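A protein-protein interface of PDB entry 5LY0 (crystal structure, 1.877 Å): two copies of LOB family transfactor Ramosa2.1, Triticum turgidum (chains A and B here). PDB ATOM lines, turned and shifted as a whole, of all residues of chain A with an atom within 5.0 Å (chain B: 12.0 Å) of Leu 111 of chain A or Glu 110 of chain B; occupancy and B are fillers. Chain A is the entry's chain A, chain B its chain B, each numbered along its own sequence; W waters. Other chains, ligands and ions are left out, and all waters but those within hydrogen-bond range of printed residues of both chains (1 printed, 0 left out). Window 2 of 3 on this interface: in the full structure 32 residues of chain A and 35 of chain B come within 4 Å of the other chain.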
ATOM      1  N   ALA A 107       5.575  28.528  23.600  1.00  0.00           N
ATOM      2  CA  ALA A 107       6.957  28.080  23.465  1.00  0.00           C
ATOM      3  C   ALA A 107       7.690  28.866  22.384  1.00  0.00           C
ATOM      4  O   ALA A 107       8.852  29.245  22.567  1.00  0.00           O
ATOM      5  CB  ALA A 107       6.998  26.583  23.164  1.00  0.00           C
ATOM      6  N   HIS A 108       7.031  29.120  21.252  1.00  0.00           N
ATOM      7  CA  HIS A 108       7.658  29.914  20.199  1.00  0.00           C
ATOM      8  C   HIS A 108       7.924  31.338  20.674  1.00  0.00           C
ATOM      9  O   HIS A 108       8.949  31.937  20.327  1.00  0.00           O
ATOM     10  CB  HIS A 108       6.779  29.917  18.949  1.00  0.00           C
ATOM     11  CG  HIS A 108       6.767  28.609  18.224  1.00  0.00           C
ATOM     12  ND1 HIS A 108       7.923  27.937  17.892  1.00  0.00           N
ATOM     13  CD2 HIS A 108       5.744  27.848  17.768  1.00  0.00           C
ATOM     14  CE1 HIS A 108       7.613  26.816  17.265  1.00  0.00           C
ATOM     15  NE2 HIS A 108       6.298  26.740  17.174  1.00  0.00           N
ATOM     16  N   THR A 109       7.011  31.893  21.475  1.00  0.00           N
ATOM     17  CA  THR A 109       7.235  33.214  22.052  1.00  0.00           C
ATOM     18  C   THR A 109       8.442  33.205  22.980  1.00  0.00           C
ATOM     19  O   THR A 109       9.267  34.124  22.951  1.00  0.00           O
ATOM     20  CB  THR A 109       5.981  33.666  22.802  1.00  0.00           C
ATOM     21  OG1 THR A 109       4.888  33.779  21.882  1.00  0.00           O
ATOM     22  CG2 THR A 109       6.202  35.014  23.486  1.00  0.00           C
ATOM     23  N   GLU A 110       8.558  32.172  23.817  1.00  0.00           N
ATOM     24  CA  GLU A 110       9.694  32.072  24.728  1.00  0.00           C
ATOM     25  C   GLU A 110      11.000  31.906  23.959  1.00  0.00           C
ATOM     26  O   GLU A 110      12.026  32.489  24.327  1.00  0.00           O
ATOM     27  CB  GLU A 110       9.470  30.906  25.695  1.00  0.00           C
ATOM     28  CG  GLU A 110      10.642  30.536  26.602  1.00  0.00           C
ATOM     29  CD  GLU A 110      10.556  31.177  27.971  1.00  0.00           C
ATOM     30  OE1 GLU A 110       9.989  32.287  28.091  1.00  0.00           O
ATOM     31  OE2 GLU A 110      11.049  30.558  28.934  1.00  0.00           O
ATOM     32  N   LEU A 111      10.979  31.116  22.883  1.00  0.00           N
ATOM     33  CA  LEU A 111      12.185  30.930  22.081  1.00  0.00           C
ATOM     34  C   LEU A 111      12.662  32.245  21.481  1.00  0.00           C
ATOM     35  O   LEU A 111      13.867  32.522  21.449  1.00  0.00           O
ATOM     36  CB  LEU A 111      11.922  29.905  20.976  1.00  0.00           C
ATOM     37  CG  LEU A 111      11.957  28.438  21.406  1.00  0.00           C
ATOM     38  CD1 LEU A 111      11.341  27.552  20.337  1.00  0.00           C
ATOM     39  CD2 LEU A 111      13.388  28.011  21.695  1.00  0.00           C
ATOM     40  N   LEU A 112      11.734  33.071  20.993  1.00  0.00           N
ATOM     41  CA  LEU A 112      12.126  34.344  20.397  1.00  0.00           C
ATOM     42  C   LEU A 112      12.764  35.263  21.430  1.00  0.00           C
ATOM     43  O   LEU A 112      13.731  35.973  21.128  1.00  0.00           O
ATOM     44  CB  LEU A 112      10.915  35.022  19.757  1.00  0.00           C
ATOM     45  CG  LEU A 112      10.523  34.572  18.348  1.00  0.00           C
ATOM     46  CD1 LEU A 112       9.262  35.301  17.924  1.00  0.00           C
ATOM     47  CD2 LEU A 112      11.647  34.818  17.347  1.00  0.00           C
ATOM     48  N   ARG A 113      12.234  35.273  22.652  1.00  0.00           N
ATOM     49  CA  ARG A 113      12.818  36.105  23.695  1.00  0.00           C
ATOM     50  C   ARG A 113      14.235  35.658  24.028  1.00  0.00           C
ATOM     51  O   ARG A 113      15.084  36.491  24.365  1.00  0.00           O
ATOM     52  CB  ARG A 113      11.934  36.075  24.939  1.00  0.00           C
ATOM     53  CG  ARG A 113      12.218  37.202  25.933  1.00  0.00           C
ATOM     54  CD  ARG A 113      11.244  37.217  27.113  1.00  0.00           C
ATOM     55  NE  ARG A 113       9.985  36.536  26.821  1.00  0.00           N
ATOM     56  CZ  ARG A 113       9.781  35.229  26.977  1.00  0.00           C
ATOM     57  NH1 ARG A 113      10.760  34.449  27.419  1.00  0.00           N
ATOM     58  NH2 ARG A 113       8.602  34.699  26.685  1.00  0.00           N
ATOM     59  N   TYR A 114      14.512  34.356  23.938  1.00  0.00           N
ATOM     60  CA  TYR A 114      15.874  33.878  24.158  1.00  0.00           C
ATOM     61  C   TYR A 114      16.821  34.410  23.090  1.00  0.00           C
ATOM     62  O   TYR A 114      17.983  34.720  23.376  1.00  0.00           O
ATOM     63  CB  TYR A 114      15.906  32.348  24.177  1.00  0.00           C
ATOM     64  CG  TYR A 114      15.723  31.735  25.549  1.00  0.00           C
ATOM     65  CD1 TYR A 114      16.623  32.000  26.574  1.00  0.00           C
ATOM     66  CD2 TYR A 114      14.663  30.878  25.815  1.00  0.00           C
ATOM     67  CE1 TYR A 114      16.466  31.440  27.828  1.00  0.00           C
ATOM     68  CE2 TYR A 114      14.498  30.310  27.067  1.00  0.00           C
ATOM     69  CZ  TYR A 114      15.403  30.597  28.068  1.00  0.00           C
ATOM     70  OH  TYR A 114      15.244  30.035  29.314  1.00  0.00           O
ATOM     71  N   ALA A 115      16.341  34.526  21.849  1.00  0.00           N
ATOM     72  CA  ALA A 115      17.198  34.983  20.762  1.00  0.00           C
ATOM     73  C   ALA A 115      17.277  36.504  20.705  1.00  0.00           C
ATOM     74  O   ALA A 115      18.341  37.062  20.415  1.00  0.00           O
ATOM     75  CB  ALA A 115      16.692  34.432  19.429  1.00  0.00           C
ATOM     76  N   LEU B 100       0.940  18.605  16.283  1.00  0.00           N
ATOM     77  CA  LEU B 100       1.278  19.608  17.287  1.00  0.00           C
ATOM     78  C   LEU B 100       2.220  19.042  18.340  1.00  0.00           C
ATOM     79  O   LEU B 100       3.140  19.733  18.793  1.00  0.00           O
ATOM     80  CB  LEU B 100       0.005  20.146  17.938  1.00  0.00           C
ATOM     81  CG  LEU B 100      -0.841  21.062  17.054  1.00  0.00           C
ATOM     82  CD1 LEU B 100      -2.212  21.275  17.669  1.00  0.00           C
ATOM     83  CD2 LEU B 100      -0.142  22.398  16.832  1.00  0.00           C
ATOM     84  N   GLN B 101       2.007  17.791  18.750  1.00  0.00           N
ATOM     85  CA  GLN B 101       2.885  17.201  19.755  1.00  0.00           C
ATOM     86  C   GLN B 101       4.297  17.036  19.212  1.00  0.00           C
ATOM     87  O   GLN B 101       5.275  17.213  19.945  1.00  0.00           O
ATOM     88  CB  GLN B 101       2.325  15.856  20.223  1.00  0.00           C
ATOM     89  CG  GLN B 101       3.068  15.262  21.411  1.00  0.00           C
ATOM     90  CD  GLN B 101       3.183  16.234  22.569  1.00  0.00           C
ATOM     91  OE1 GLN B 101       2.203  16.515  23.259  1.00  0.00           O
ATOM     92  NE2 GLN B 101       4.384  16.764  22.778  1.00  0.00           N
ATOM     93  N   LYS B 102       4.422  16.704  17.927  1.00  0.00           N
ATOM     94  CA  LYS B 102       5.736  16.641  17.299  1.00  0.00           C
ATOM     95  C   LYS B 102       6.407  18.008  17.317  1.00  0.00           C
ATOM     96  O   LYS B 102       7.587  18.135  17.667  1.00  0.00           O
ATOM     97  CB  LYS B 102       5.595  16.127  15.865  1.00  0.00           C
ATOM     98  CG  LYS B 102       6.910  15.729  15.210  1.00  0.00           C
ATOM     99  CD  LYS B 102       6.752  14.466  14.378  1.00  0.00           C
ATOM    100  CE  LYS B 102       6.548  13.236  15.257  1.00  0.00           C
ATOM    101  NZ  LYS B 102       6.253  12.017  14.459  1.00  0.00           N
ATOM    102  N   GLU B 103       5.661  19.048  16.943  1.00  0.00           N
ATOM    103  CA  GLU B 103       6.208  20.400  16.943  1.00  0.00           C
ATOM    104  C   GLU B 103       6.597  20.834  18.351  1.00  0.00           C
ATOM    105  O   GLU B 103       7.626  21.492  18.545  1.00  0.00           O
ATOM    106  CB  GLU B 103       5.184  21.360  16.336  1.00  0.00           C
ATOM    107  CG  GLU B 103       5.777  22.615  15.711  1.00  0.00           C
ATOM    108  CD  GLU B 103       4.825  23.285  14.734  1.00  0.00           C
ATOM    109  OE1 GLU B 103       3.870  22.621  14.279  1.00  0.00           O
ATOM    110  OE2 GLU B 103       5.030  24.478  14.425  1.00  0.00           O
ATOM    111  N   LEU B 104       5.789  20.468  19.349  1.00  0.00           N
ATOM    112  CA  LEU B 104       6.101  20.839  20.726  1.00  0.00           C
ATOM    113  C   LEU B 104       7.352  20.129  21.221  1.00  0.00           C
ATOM    114  O   LEU B 104       8.136  20.706  21.983  1.00  0.00           O
ATOM    115  CB  LEU B 104       4.918  20.525  21.641  1.00  0.00           C
ATOM    116  CG  LEU B 104       3.919  21.656  21.892  1.00  0.00           C
ATOM    117  CD1 LEU B 104       2.722  21.115  22.651  1.00  0.00           C
ATOM    118  CD2 LEU B 104       4.565  22.802  22.661  1.00  0.00           C
ATOM    119  N   ASP B 105       7.548  18.872  20.817  1.00  0.00           N
ATOM    120  CA  ASP B 105       8.773  18.169  21.177  1.00  0.00           C
ATOM    121  C   ASP B 105       9.991  18.987  20.776  1.00  0.00           C
ATOM    122  O   ASP B 105      10.851  19.293  21.606  1.00  0.00           O
ATOM    123  CB  ASP B 105       8.812  16.791  20.515  1.00  0.00           C
ATOM    124  CG  ASP B 105       7.621  15.933  20.887  1.00  0.00           C
ATOM    125  OD1 ASP B 105       7.029  16.170  21.961  1.00  0.00           O
ATOM    126  OD2 ASP B 105       7.276  15.019  20.105  1.00  0.00           O
ATOM    127  N   ALA B 106      10.063  19.378  19.502  1.00  0.00           N
ATOM    128  CA  ALA B 106      11.201  20.160  19.031  1.00  0.00           C
ATOM    129  C   ALA B 106      11.349  21.452  19.824  1.00  0.00           C
ATOM    130  O   ALA B 106      12.462  21.833  20.205  1.00  0.00           O
ATOM    131  CB  ALA B 106      11.044  20.459  17.540  1.00  0.00           C
ATOM    132  N   ALA B 107      10.236  22.135  20.090  1.00  0.00           N
ATOM    133  CA  ALA B 107      10.301  23.410  20.796  1.00  0.00           C
ATOM    134  C   ALA B 107      10.806  23.232  22.224  1.00  0.00           C
ATOM    135  O   ALA B 107      11.639  24.014  22.696  1.00  0.00           O
ATOM    136  CB  ALA B 107       8.927  24.079  20.794  1.00  0.00           C
ATOM    137  N   HIS B 108      10.317  22.207  22.926  1.00  0.00           N
ATOM    138  CA  HIS B 108      10.716  22.010  24.317  1.00  0.00           C
ATOM    139  C   HIS B 108      12.203  21.690  24.431  1.00  0.00           C
ATOM    140  O   HIS B 108      12.878  22.172  25.350  1.00  0.00           O
ATOM    141  CB  HIS B 108       9.879  20.899  24.951  1.00  0.00           C
ATOM    142  CG  HIS B 108       8.483  21.317  25.299  1.00  0.00           C
ATOM    143  ND1 HIS B 108       7.447  20.417  25.427  1.00  0.00           N
ATOM    144  CD2 HIS B 108       7.953  22.537  25.554  1.00  0.00           C
ATOM    145  CE1 HIS B 108       6.339  21.064  25.742  1.00  0.00           C
ATOM    146  NE2 HIS B 108       6.619  22.352  25.826  1.00  0.00           N
ATOM    147  N   THR B 109      12.732  20.880  23.513  1.00  0.00           N
ATOM    148  CA  THR B 109      14.158  20.568  23.555  1.00  0.00           C
ATOM    149  C   THR B 109      14.990  21.806  23.249  1.00  0.00           C
ATOM    150  O   THR B 109      16.024  22.043  23.886  1.00  0.00           O
ATOM    151  CB  THR B 109      14.495  19.447  22.569  1.00  0.00           C
ATOM    152  OG1 THR B 109      14.397  19.942  21.228  1.00  0.00           O
ATOM    153  CG2 THR B 109      13.555  18.260  22.748  1.00  0.00           C
ATOM    154  N   GLU B 110      14.554  22.607  22.276  1.00  0.00           N
ATOM    155  CA  GLU B 110      15.227  23.870  21.988  1.00  0.00           C
ATOM    156  C   GLU B 110      15.245  24.764  23.222  1.00  0.00           C
ATOM    157  O   GLU B 110      16.280  25.345  23.571  1.00  0.00           O
ATOM    158  CB  GLU B 110      14.526  24.574  20.825  1.00  0.00           C
ATOM    159  CG  GLU B 110      15.341  25.673  20.164  1.00  0.00           C
ATOM    160  CD  GLU B 110      16.206  25.154  19.035  1.00  0.00           C
ATOM    161  OE1 GLU B 110      16.577  23.963  19.070  1.00  0.00           O
ATOM    162  OE2 GLU B 110      16.511  25.938  18.110  1.00  0.00           O
ATOM    163  N   LEU B 111      14.100  24.878  23.898  1.00  0.00           N
ATOM    164  CA  LEU B 111      14.017  25.704  25.097  1.00  0.00           C
ATOM    165  C   LEU B 111      14.904  25.160  26.206  1.00  0.00           C
ATOM    166  O   LEU B 111      15.542  25.929  26.935  1.00  0.00           O
ATOM    167  CB  LEU B 111      12.565  25.784  25.567  1.00  0.00           C
ATOM    168  CG  LEU B 111      11.665  26.695  24.739  1.00  0.00           C
ATOM    169  CD1 LEU B 111      10.206  26.496  25.128  1.00  0.00           C
ATOM    170  CD2 LEU B 111      12.091  28.136  24.940  1.00  0.00           C
ATOM    171  N   LEU B 112      14.948  23.837  26.359  1.00  0.00           N
ATOM    172  CA  LEU B 112      15.790  23.253  27.394  1.00  0.00           C
ATOM    173  C   LEU B 112      17.259  23.569  27.144  1.00  0.00           C
ATOM    174  O   LEU B 112      18.013  23.840  28.085  1.00  0.00           O
ATOM    175  CB  LEU B 112      15.563  21.743  27.458  1.00  0.00           C
ATOM    176  CG  LEU B 112      16.376  20.976  28.503  1.00  0.00           C
ATOM    177  CD1 LEU B 112      16.151  21.550  29.897  1.00  0.00           C
ATOM    178  CD2 LEU B 112      16.015  19.501  28.461  1.00  0.00           C
ATOM    179  N   ARG B 113      17.679  23.554  25.877  1.00  0.00           N
ATOM    180  CA  ARG B 113      19.059  23.902  25.554  1.00  0.00           C
ATOM    181  C   ARG B 113      19.355  25.354  25.912  1.00  0.00           C
ATOM    182  O   ARG B 113      20.427  25.665  26.444  1.00  0.00           O
ATOM    183  CB  ARG B 113      19.330  23.645  24.070  1.00  0.00           C
ATOM    184  CG  ARG B 113      20.740  24.009  23.629  1.00  0.00           C
ATOM    185  CD  ARG B 113      21.063  23.450  22.249  1.00  0.00           C
ATOM    186  NE  ARG B 113      20.024  23.746  21.268  1.00  0.00           N
ATOM    187  CZ  ARG B 113      20.053  23.345  20.001  1.00  0.00           C
ATOM    188  NH1 ARG B 113      21.071  22.626  19.547  1.00  0.00           N
ATOM    189  NH2 ARG B 113      19.059  23.663  19.185  1.00  0.00           N
ATOM    190  N   TYR B 114      18.415  26.259  25.629  1.00  0.00           N
ATOM    191  CA  TYR B 114      18.590  27.654  26.023  1.00  0.00           C
ATOM    192  C   TYR B 114      18.657  27.791  27.539  1.00  0.00           C
ATOM    193  O   TYR B 114      19.484  28.545  28.064  1.00  0.00           O
ATOM    194  CB  TYR B 114      17.449  28.509  25.472  1.00  0.00           C
ATOM    195  CG  TYR B 114      17.661  29.020  24.064  1.00  0.00           C
ATOM    196  CD1 TYR B 114      18.641  29.964  23.787  1.00  0.00           C
ATOM    197  CD2 TYR B 114      16.863  28.578  23.015  1.00  0.00           C
ATOM    198  CE1 TYR B 114      18.832  30.443  22.503  1.00  0.00           C
ATOM    199  CE2 TYR B 114      17.047  29.051  21.729  1.00  0.00           C
ATOM    200  CZ  TYR B 114      18.031  29.983  21.479  1.00  0.00           C
ATOM    201  OH  TYR B 114      18.217  30.458  20.201  1.00  0.00           O
ATOM    202  N   ALA B 115      17.792  27.074  28.257  1.00  0.00           N
ATOM    203  CA  ALA B 115      17.768  27.177  29.712  1.00  0.00           C
ATOM    204  C   ALA B 115      19.090  26.737  30.328  1.00  0.00           C
ATOM    205  O   ALA B 115      19.464  27.216  31.402  1.00  0.00           O
ATOM    206  CB  ALA B 115      16.623  26.342  30.280  1.00  0.00           C
ATOM    207  N   CYS B 116      19.811  25.830  29.667  1.00  0.00           N
ATOM    208  CA  CYS B 116      21.092  25.352  30.170  1.00  0.00           C
ATOM    209  C   CYS B 116      22.255  26.273  29.809  1.00  0.00           C
ATOM    210  O   CYS B 116      23.410  25.858  29.939  1.00  0.00           O
ATOM    211  CB  CYS B 116      21.368  23.941  29.641  1.00  0.00           C
ATOM    212  SG  CYS B 116      20.263  22.672  30.298  1.00  0.00           S
ATOM    213  N   GLY B 117      21.982  27.496  29.362  1.00  0.00           N
ATOM    214  CA  GLY B 117      23.022  28.464  29.084  1.00  0.00           C
ATOM    215  C   GLY B 117      23.208  28.762  27.619  1.00  0.00           C
ATOM    216  O   GLY B 117      24.238  29.312  27.208  1.00  0.00           O
HETATM  217  O   HOH W   1      13.459  27.608  28.995  1.00  0.00           O
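OE1 of Glu 110 of chain A is in salt-bridge range of NH2 of Arg 113 of chain A (3.1 Å).
OE1 of Glu 110 of chain B lies within salt-bridge range of NH2 of Arg 113 of chain B, at 2.5 Å.
Of the 9 printed residues of chain A, 5 touch a printed residue of chain B.
Hydrophobic or aromatic side chains of chain A within 4 Å of the printed part of chain B: Ala 107, His 108, Leu 111 and Tyr 114.
Among the printed residues, no Asp or Glu carboxylate lies within 4 Å of a Lys or Arg side-chain nitrogen of the other chain.
Of chain B, only Glu 110, Leu 111 and Tyr 114 come within 4 Å of Leu 111 of chain A.
His 108 of chain A touches just one residue of chain B: Glu 103 (3.8 Å).
No residue of chain B comes within 4 Å of Thr 109 of chain A.
Glu 110 of chain A touches one residue of chain B.
No residue of chain B comes within 4 Å of Arg 113 of chain A.
Tyr 114 of chain A touches just these residues of chain B: Leu 111, Tyr 114 and Ala 115.
No residue of chain B comes within 4 Å of Ala 115 of chain A.
Of the printed residues of chain A, Leu 111 of chain B touches Ala 107 (3.8 Å), Glu 110 (3.3 Å), Leu 111 (3.5 Å) and Tyr 114 (3.9 Å).
Of the printed residues of chain A, Ala 107 of chain B touches Ala 107.
Printed residues of chain A within 4 Å of Ala 115 of chain B: Tyr 114 (3.8 Å).
Asp 105 of chain B touches none of the printed residues of chain A.
Gln 101 of chain B touches none of the printed residues of chain A.
The nearest printed residue of chain A that does not touch Glu 110 of chain B is Tyr 114 of chain A (6.2 Å).
The nearest printed residue of chain A that does not touch Glu 103 of chain B is Ala 107 of chain A (6.9 Å).
Among the printed residues, merely in contact across the chains: Ala 107 of chain A with Ala 107 of chain B (3.95 Å), Ala 107 of chain A with Leu 111 of chain B (3.8 Å), His 108 of chain A with Glu 103 of chain B (3.8 Å), Glu 110 of chain A with Leu 111 of chain B (3.3 Å), Leu 111 of chain A with Glu 110 of chain B (3.4 Å), Leu 111 of chain A with Leu 111 of chain B (3.5 Å), Leu 111 of chain A with Tyr 114 of chain B (3.8 Å), Tyr 114 of chain A with Leu 111 of chain B (3.9 Å), Tyr 114 of chain A with Tyr 114 of chain B (3.6 Å) and Tyr 114 of chain A with Ala 115 of chain B (3.8 Å).
Ala 107 of chain B touches its own counterpart, Ala 107 of chain A.
Ala 107 of chain A touches Leu 111 of chain B, but with the chains exchanged Leu 111 of chain A does not touch Ala 107 of chain B (4.3 Å).
Glu 110 of chain A touches Leu 111 of chain B, and with the chains exchanged Leu 111 of chain A touches Glu 110 of chain B.
Tyr 114 of chain B touches its own counterpart, Tyr 114 of chain A.
Of the 10 pairs that touch across the chains among the printed residues, 7 have their exchanged pair printed and touching as well.
Water W1 lies within hydrogen-bond range of OH of Tyr 114 of chain A (3.0 Å) and O of Leu 111 of chain B (3.4 Å).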
